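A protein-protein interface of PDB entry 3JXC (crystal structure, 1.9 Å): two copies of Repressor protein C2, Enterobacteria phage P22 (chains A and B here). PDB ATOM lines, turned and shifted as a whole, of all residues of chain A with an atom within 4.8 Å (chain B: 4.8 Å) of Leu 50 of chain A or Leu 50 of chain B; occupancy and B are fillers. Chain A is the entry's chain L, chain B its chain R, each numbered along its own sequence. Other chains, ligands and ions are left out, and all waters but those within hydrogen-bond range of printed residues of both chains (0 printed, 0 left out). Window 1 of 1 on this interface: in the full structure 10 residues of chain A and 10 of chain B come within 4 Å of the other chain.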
ATOM      1  N   GLY A  46       6.418  -0.453  -6.043  1.00  0.00           N
ATOM      2  CA  GLY A  46       5.012  -0.919  -6.014  1.00  0.00           C
ATOM      3  C   GLY A  46       4.856  -2.308  -6.645  1.00  0.00           C
ATOM      4  O   GLY A  46       4.341  -3.245  -6.021  1.00  0.00           O
ATOM      5  N   GLU A  47       5.340  -2.431  -7.871  1.00  0.00           N
ATOM      6  CA  GLU A  47       5.292  -3.687  -8.639  1.00  0.00           C
ATOM      7  C   GLU A  47       6.015  -4.826  -7.918  1.00  0.00           C
ATOM      8  O   GLU A  47       5.517  -5.972  -7.869  1.00  0.00           O
ATOM      9  CB  GLU A  47       5.942  -3.445  -9.996  1.00  0.00           C
ATOM     10  CG  GLU A  47       6.059  -4.652 -10.875  1.00  0.00           C
ATOM     11  CD  GLU A  47       6.637  -4.310 -12.229  1.00  0.00           C
ATOM     12  OE1 GLU A  47       7.792  -3.828 -12.292  1.00  0.00           O
ATOM     13  OE2 GLU A  47       5.933  -4.528 -13.240  1.00  0.00           O
ATOM     14  N   ASN A  48       7.189  -4.507  -7.364  1.00  0.00           N
ATOM     15  CA  ASN A  48       8.019  -5.505  -6.718  1.00  0.00           C
ATOM     16  C   ASN A  48       7.448  -5.952  -5.376  1.00  0.00           C
ATOM     17  O   ASN A  48       7.577  -7.134  -5.008  1.00  0.00           O
ATOM     18  CB  ASN A  48       9.476  -5.032  -6.604  1.00  0.00           C
ATOM     19  CG  ASN A  48      10.181  -4.979  -7.964  1.00  0.00           C
ATOM     20  OD1 ASN A  48       9.760  -5.637  -8.920  1.00  0.00           O
ATOM     21  ND2 ASN A  48      11.237  -4.164  -8.070  1.00  0.00           N
ATOM     22  N   LEU A  49       6.822  -5.028  -4.650  1.00  0.00           N
ATOM     23  CA  LEU A  49       6.253  -5.376  -3.346  1.00  0.00           C
ATOM     24  C   LEU A  49       5.129  -6.402  -3.549  1.00  0.00           C
ATOM     25  O   LEU A  49       5.003  -7.360  -2.772  1.00  0.00           O
ATOM     26  CB  LEU A  49       5.703  -4.156  -2.608  1.00  0.00           C
ATOM     27  CG  LEU A  49       4.965  -4.391  -1.264  1.00  0.00           C
ATOM     28  CD1 LEU A  49       5.834  -5.090  -0.216  1.00  0.00           C
ATOM     29  CD2 LEU A  49       4.460  -3.075  -0.712  1.00  0.00           C
ATOM     30  N   LEU A  50       4.310  -6.167  -4.573  1.00  0.00           N
ATOM     31  CA  LEU A  50       3.153  -7.044  -4.839  1.00  0.00           C
ATOM     32  C   LEU A  50       3.642  -8.410  -5.328  1.00  0.00           C
ATOM     33  O   LEU A  50       3.156  -9.448  -4.860  1.00  0.00           O
ATOM     34  CB  LEU A  50       2.168  -6.366  -5.801  1.00  0.00           C
ATOM     35  CG  LEU A  50       1.065  -5.510  -5.140  1.00  0.00           C
ATOM     36  CD1 LEU A  50      -0.022  -6.400  -4.549  1.00  0.00           C
ATOM     37  CD2 LEU A  50       1.570  -4.591  -4.049  1.00  0.00           C
ATOM     38  N   ALA A  51       4.650  -8.420  -6.199  1.00  0.00           N
ATOM     39  CA  ALA A  51       5.282  -9.686  -6.632  1.00  0.00           C
ATOM     40  C   ALA A  51       5.927 -10.443  -5.471  1.00  0.00           C
ATOM     41  O   ALA A  51       5.819 -11.680  -5.370  1.00  0.00           O
ATOM     42  CB  ALA A  51       6.310  -9.443  -7.785  1.00  0.00           C
ATOM     43  N   LEU A  52       6.583  -9.703  -4.582  1.00  0.00           N
ATOM     44  CA  LEU A  52       7.235 -10.273  -3.404  1.00  0.00           C
ATOM     45  C   LEU A  52       6.208 -10.888  -2.446  1.00  0.00           C
ATOM     46  O   LEU A  52       6.404 -11.999  -1.927  1.00  0.00           O
ATOM     47  CB  LEU A  52       8.026  -9.180  -2.661  1.00  0.00           C
ATOM     48  CG  LEU A  52       8.715  -9.537  -1.350  1.00  0.00           C
ATOM     49  CD1 LEU A  52       9.816 -10.607  -1.595  1.00  0.00           C
ATOM     50  CD2 LEU A  52       9.287  -8.278  -0.648  1.00  0.00           C
ATOM     51  N   SER A  53       5.127 -10.159  -2.205  1.00  0.00           N
ATOM     52  CA  SER A  53       4.066 -10.660  -1.333  1.00  0.00           C
ATOM     53  C   SER A  53       3.452 -11.987  -1.848  1.00  0.00           C
ATOM     54  O   SER A  53       3.156 -12.881  -1.053  1.00  0.00           O
ATOM     55  CB  SER A  53       3.003  -9.590  -1.120  1.00  0.00           C
ATOM     56  OG  SER A  53       2.248  -9.408  -2.309  1.00  0.00           O
ATOM     57  N   LYS A  54       3.287 -12.117  -3.160  1.00  0.00           N
ATOM     58  CA  LYS A  54       2.767 -13.369  -3.756  1.00  0.00           C
ATOM     59  C   LYS A  54       3.766 -14.517  -3.658  1.00  0.00           C
ATOM     60  O   LYS A  54       3.388 -15.654  -3.353  1.00  0.00           O
ATOM     61  CB  LYS A  54       2.336 -13.157  -5.199  1.00  0.00           C
ATOM     62  CG  LYS A  54       1.138 -12.239  -5.287  1.00  0.00           C
ATOM     63  CD  LYS A  54       0.733 -11.954  -6.707  1.00  0.00           C
ATOM     64  CE  LYS A  54      -0.416 -10.962  -6.700  1.00  0.00           C
ATOM     65  NZ  LYS A  54      -0.063  -9.774  -5.858  1.00  0.00           N
ATOM     66  N   PRO A  60       0.865  -7.658   1.183  1.00  0.00           N
ATOM     67  CA  PRO A  60       1.799  -6.520   1.202  1.00  0.00           C
ATOM     68  C   PRO A  60       1.729  -5.748   2.518  1.00  0.00           C
ATOM     69  O   PRO A  60       2.754  -5.300   3.023  1.00  0.00           O
ATOM     70  CB  PRO A  60       1.304  -5.636   0.056  1.00  0.00           C
ATOM     71  CG  PRO A  60       0.511  -6.529  -0.818  1.00  0.00           C
ATOM     72  CD  PRO A  60      -0.115  -7.542   0.088  1.00  0.00           C
ATOM     73  N   ASP A  61       0.526  -5.614   3.069  1.00  0.00           N
ATOM     74  CA  ASP A  61       0.334  -4.937   4.355  1.00  0.00           C
ATOM     75  C   ASP A  61       1.112  -5.599   5.480  1.00  0.00           C
ATOM     76  O   ASP A  61       1.723  -4.902   6.307  1.00  0.00           O
ATOM     77  CB  ASP A  61      -1.143  -4.904   4.713  1.00  0.00           C
ATOM     78  CG  ASP A  61      -1.986  -4.399   3.579  1.00  0.00           C
ATOM     79  OD1 ASP A  61      -2.294  -3.188   3.620  1.00  0.00           O
ATOM     80  OD2 ASP A  61      -2.291  -5.201   2.635  1.00  0.00           O
ATOM     81  N   LEU A  64       4.780  -4.683   4.968  1.00  0.00           N
ATOM     82  CA  LEU A  64       5.067  -3.258   5.237  1.00  0.00           C
ATOM     83  C   LEU A  64       4.985  -2.914   6.719  1.00  0.00           C
ATOM     84  O   LEU A  64       5.852  -2.201   7.260  1.00  0.00           O
ATOM     85  CB  LEU A  64       4.074  -2.366   4.496  1.00  0.00           C
ATOM     86  CG  LEU A  64       4.308  -2.088   3.014  1.00  0.00           C
ATOM     87  CD1 LEU A  64       3.097  -1.340   2.438  1.00  0.00           C
ATOM     88  CD2 LEU A  64       5.616  -1.282   2.821  1.00  0.00           C
ATOM     89  N   GLY B  46       6.336   1.045  -2.890  1.00  0.00           N
ATOM     90  CA  GLY B  46       5.555   0.022  -2.177  1.00  0.00           C
ATOM     91  C   GLY B  46       4.588   0.590  -1.166  1.00  0.00           C
ATOM     92  O   GLY B  46       3.362   0.361  -1.241  1.00  0.00           O
ATOM     93  N   GLU B  47       5.125   1.358  -0.223  1.00  0.00           N
ATOM     94  CA  GLU B  47       4.307   2.034   0.773  1.00  0.00           C
ATOM     95  C   GLU B  47       3.228   2.924   0.131  1.00  0.00           C
ATOM     96  O   GLU B  47       2.067   2.917   0.572  1.00  0.00           O
ATOM     97  CB  GLU B  47       5.218   2.892   1.659  1.00  0.00           C
ATOM     98  CG  GLU B  47       4.512   3.672   2.723  1.00  0.00           C
ATOM     99  CD  GLU B  47       5.494   4.276   3.718  1.00  0.00           C
ATOM    100  OE1 GLU B  47       5.132   4.394   4.911  1.00  0.00           O
ATOM    101  OE2 GLU B  47       6.617   4.644   3.300  1.00  0.00           O
ATOM    102  N   ASN B  48       3.603   3.675  -0.908  1.00  0.00           N
ATOM    103  CA  ASN B  48       2.660   4.624  -1.514  1.00  0.00           C
ATOM    104  C   ASN B  48       1.582   3.929  -2.326  1.00  0.00           C
ATOM    105  O   ASN B  48       0.444   4.387  -2.367  1.00  0.00           O
ATOM    106  CB  ASN B  48       3.381   5.706  -2.338  1.00  0.00           C
ATOM    107  CG  ASN B  48       4.252   6.618  -1.467  1.00  0.00           C
ATOM    108  OD1 ASN B  48       4.020   6.741  -0.259  1.00  0.00           O
ATOM    109  ND2 ASN B  48       5.250   7.240  -2.068  1.00  0.00           N
ATOM    110  N   LEU B  49       1.939   2.823  -2.965  1.00  0.00           N
ATOM    111  CA  LEU B  49       0.969   2.064  -3.726  1.00  0.00           C
ATOM    112  C   LEU B  49      -0.134   1.551  -2.800  1.00  0.00           C
ATOM    113  O   LEU B  49      -1.320   1.684  -3.113  1.00  0.00           O
ATOM    114  CB  LEU B  49       1.627   0.924  -4.521  1.00  0.00           C
ATOM    115  CG  LEU B  49       0.610   0.038  -5.281  1.00  0.00           C
ATOM    116  CD1 LEU B  49      -0.185   0.833  -6.349  1.00  0.00           C
ATOM    117  CD2 LEU B  49       1.322  -1.149  -5.907  1.00  0.00           C
ATOM    118  N   LEU B  50       0.262   0.979  -1.668  1.00  0.00           N
ATOM    119  CA  LEU B  50      -0.693   0.521  -0.658  1.00  0.00           C
ATOM    120  C   LEU B  50      -1.567   1.640  -0.103  1.00  0.00           C
ATOM    121  O   LEU B  50      -2.778   1.465  -0.038  1.00  0.00           O
ATOM    122  CB  LEU B  50      -0.001  -0.283   0.452  1.00  0.00           C
ATOM    123  CG  LEU B  50       0.169  -1.781   0.161  1.00  0.00           C
ATOM    124  CD1 LEU B  50      -1.178  -2.478   0.345  1.00  0.00           C
ATOM    125  CD2 LEU B  50       0.712  -2.108  -1.250  1.00  0.00           C
ATOM    126  N   ALA B  51      -0.969   2.791   0.242  1.00  0.00           N
ATOM    127  CA  ALA B  51      -1.734   3.957   0.706  1.00  0.00           C
ATOM    128  C   ALA B  51      -2.707   4.477  -0.350  1.00  0.00           C
ATOM    129  O   ALA B  51      -3.867   4.828  -0.029  1.00  0.00           O
ATOM    130  CB  ALA B  51      -0.806   5.066   1.168  1.00  0.00           C
ATOM    131  N   LEU B  52      -2.244   4.520  -1.601  1.00  0.00           N
ATOM    132  CA  LEU B  52      -3.066   4.939  -2.726  1.00  0.00           C
ATOM    133  C   LEU B  52      -4.254   3.991  -2.934  1.00  0.00           C
ATOM    134  O   LEU B  52      -5.383   4.440  -3.089  1.00  0.00           O
ATOM    135  CB  LEU B  52      -2.231   5.011  -4.015  1.00  0.00           C
ATOM    136  CG  LEU B  52      -2.946   5.415  -5.308  1.00  0.00           C
ATOM    137  CD1 LEU B  52      -3.507   6.848  -5.243  1.00  0.00           C
ATOM    138  CD2 LEU B  52      -1.970   5.231  -6.501  1.00  0.00           C
ATOM    139  N   SER B  53      -3.988   2.695  -2.947  1.00  0.00           N
ATOM    140  CA  SER B  53      -5.054   1.710  -3.168  1.00  0.00           C
ATOM    141  C   SER B  53      -6.151   1.838  -2.087  1.00  0.00           C
ATOM    142  O   SER B  53      -7.338   1.819  -2.409  1.00  0.00           O
ATOM    143  CB  SER B  53      -4.470   0.292  -3.310  1.00  0.00           C
ATOM    144  OG  SER B  53      -4.146  -0.291  -2.064  1.00  0.00           O
ATOM    145  N   LYS B  54      -5.746   2.068  -0.837  1.00  0.00           N
ATOM    146  CA  LYS B  54      -6.696   2.327   0.251  1.00  0.00           C
ATOM    147  C   LYS B  54      -7.516   3.598   0.036  1.00  0.00           C
ATOM    148  O   LYS B  54      -8.753   3.560   0.094  1.00  0.00           O
ATOM    149  CB  LYS B  54      -5.995   2.346   1.605  1.00  0.00           C
ATOM    150  CG  LYS B  54      -5.664   0.949   2.103  1.00  0.00           C
ATOM    151  CD  LYS B  54      -4.852   1.008   3.385  1.00  0.00           C
ATOM    152  CE  LYS B  54      -4.266  -0.358   3.762  1.00  0.00           C
ATOM    153  NZ  LYS B  54      -3.593  -1.055   2.614  1.00  0.00           N
ATOM    154  N   PRO B  60      -4.250  -3.037  -4.819  1.00  0.00           N
ATOM    155  CA  PRO B  60      -3.019  -2.644  -5.508  1.00  0.00           C
ATOM    156  C   PRO B  60      -2.886  -3.335  -6.861  1.00  0.00           C
ATOM    157  O   PRO B  60      -2.417  -2.739  -7.821  1.00  0.00           O
ATOM    158  CB  PRO B  60      -1.898  -3.130  -4.566  1.00  0.00           C
ATOM    159  CG  PRO B  60      -2.544  -3.370  -3.242  1.00  0.00           C
ATOM    160  CD  PRO B  60      -3.989  -3.660  -3.508  1.00  0.00           C
ATOM    161  N   ASP B  61      -3.306  -4.602  -6.939  1.00  0.00           N
ATOM    162  CA  ASP B  61      -3.278  -5.315  -8.220  1.00  0.00           C
ATOM    163  C   ASP B  61      -4.149  -4.678  -9.297  1.00  0.00           C
ATOM    164  O   ASP B  61      -3.740  -4.609 -10.457  1.00  0.00           O
ATOM    165  CB  ASP B  61      -3.610  -6.796  -8.031  1.00  0.00           C
ATOM    166  CG  ASP B  61      -2.451  -7.566  -7.437  1.00  0.00           C
ATOM    167  OD1 ASP B  61      -2.583  -8.023  -6.296  1.00  0.00           O
ATOM    168  OD2 ASP B  61      -1.395  -7.677  -8.098  1.00  0.00           O
ATOM    169  N   LEU B  64      -2.157  -1.761 -10.604  1.00  0.00           N
ATOM    170  CA  LEU B  64      -0.943  -2.198 -11.299  1.00  0.00           C
ATOM    171  C   LEU B  64      -1.231  -2.852 -12.642  1.00  0.00           C
ATOM    172  O   LEU B  64      -0.566  -2.568 -13.636  1.00  0.00           O
ATOM    173  CB  LEU B  64      -0.150  -3.181 -10.432  1.00  0.00           C
ATOM    174  CG  LEU B  64       0.777  -2.685  -9.329  1.00  0.00           C
ATOM    175  CD1 LEU B  64       1.215  -3.878  -8.476  1.00  0.00           C
ATOM    176  CD2 LEU B  64       1.988  -1.912  -9.931  1.00  0.00           C
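OD1 of Asp 61 of chain B lies within salt-bridge range of NZ of Lys 54 of chain A, 3.1 Å away.
The side-chain carboxylate (OD1) of Asp 61 of chain A lies within salt-bridge range of the side-chain amino group (NZ) of Lys 54 of chain B.
N of Gly 46 of chain B lies close to N of Gly 46 of chain A (3.5 Å).
The side-chain hydroxyl (OG) of Ser 53 of chain A lies close to the backbone carbonyl oxygen (O) of Leu 49 of chain A (3.5 Å).
The side-chain hydroxyl of Ser 53 of chain A is in hydrogen-bond range of the backbone carbonyl oxygen of Leu 50 of chain A, 2.7 Å away.
The side-chain amino group (NZ) of Lys 54 of chain A is in hydrogen-bond range of the backbone carbonyl oxygen (O) of Leu 50 of chain A (3.4 Å).
O of Leu 50 of chain B sits at hydrogen-bond distance from OG of Ser 53 of chain B (3.0 Å).
Among the printed residues, pairs that only touch across the chains: Gly 46 of chain A with Leu 49 of chain B, Glu 47 of chain A with Leu 64 of chain B, Leu 49 of chain A with Gly 46 of chain B, Leu 49 of chain A with Leu 50 of chain B, Leu 50 of chain A with Leu 49 of chain B, Leu 50 of chain A with Leu 50 of chain B, Leu 50 of chain A with Pro 60 of chain B, Leu 50 of chain A with Asp 61 of chain B, Leu 50 of chain A with Leu 64 of chain B, Pro 60 of chain A with Leu 50 of chain B, Asp 61 of chain A with Leu 50 of chain B, Leu 64 of chain A with Glu 47 of chain B and Leu 64 of chain A with Leu 50 of chain B.
Leu 50 of chain A touches just these residues of chain B: Leu 49, Leu 50, Pro 60, Asp 61 and Leu 64.
Of chain A, only Leu 49 (3.9 Å), Leu 50 (3.8 Å), Pro 60 (3.8 Å), Asp 61 (3.5 Å) and Leu 64 (3.7 Å) come within 4 Å of Leu 50 of chain B.
Printed residues of chain B within 4 Å of Leu 64 of chain A: Glu 47 (3.95 Å) and Leu 50 (3.7 Å).
Of the printed residues of chain A, Lys 54 of chain B touches Asp 61.
Printed residues of chain B within 4 Å of Pro 60 of chain A: Leu 50 (3.8 Å).
Ala 51 of chain B touches none of the printed residues of chain A.
Ala 51 of chain A touches none of the printed residues of chain B.
The nearest printed residue of chain B that does not touch Leu 50 of chain A is Gly 46 of chain B (6.0 Å).
The nearest printed residue of chain A that does not touch Leu 50 of chain B is Gly 46 of chain A (6.1 Å).
The nearest printed residue of chain A that does not touch Lys 54 of chain B is Leu 64 of chain A (6.7 Å).
Of the 12 printed residues of chain B, 8 touch a printed residue of chain A.
Hydrophobic or aromatic side chains of chain B that line the printed part of chain A: Leu 49, Leu 50, Pro 60 and Leu 64.
Hydrophobic or aromatic side chains of chain A within 4 Å of the printed part of chain B: Leu 49, Leu 50, Pro 60 and Leu 64.
Along chain A the printed residues that touch a printed residue of chain B span positions 46 to 64.
Glu 47 of chain A touches Leu 64 of chain B, and with the chains exchanged Leu 64 of chain A touches Glu 47 of chain B.
Leu 50 of chain A touches Pro 60 of chain B, and with the chains exchanged Pro 60 of chain A touches Leu 50 of chain B.
Leu 50 of chain A touches Asp 61 of chain B, and with the chains exchanged Asp 61 of chain A touches Leu 50 of chain B.
Lys 54 of chain A touches Asp 61 of chain B, and with the chains exchanged Asp 61 of chain A touches Lys 54 of chain B.
Of the 16 pairs that touch across the chains among the printed residues, 16 have their exchanged pair printed and touching as well.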
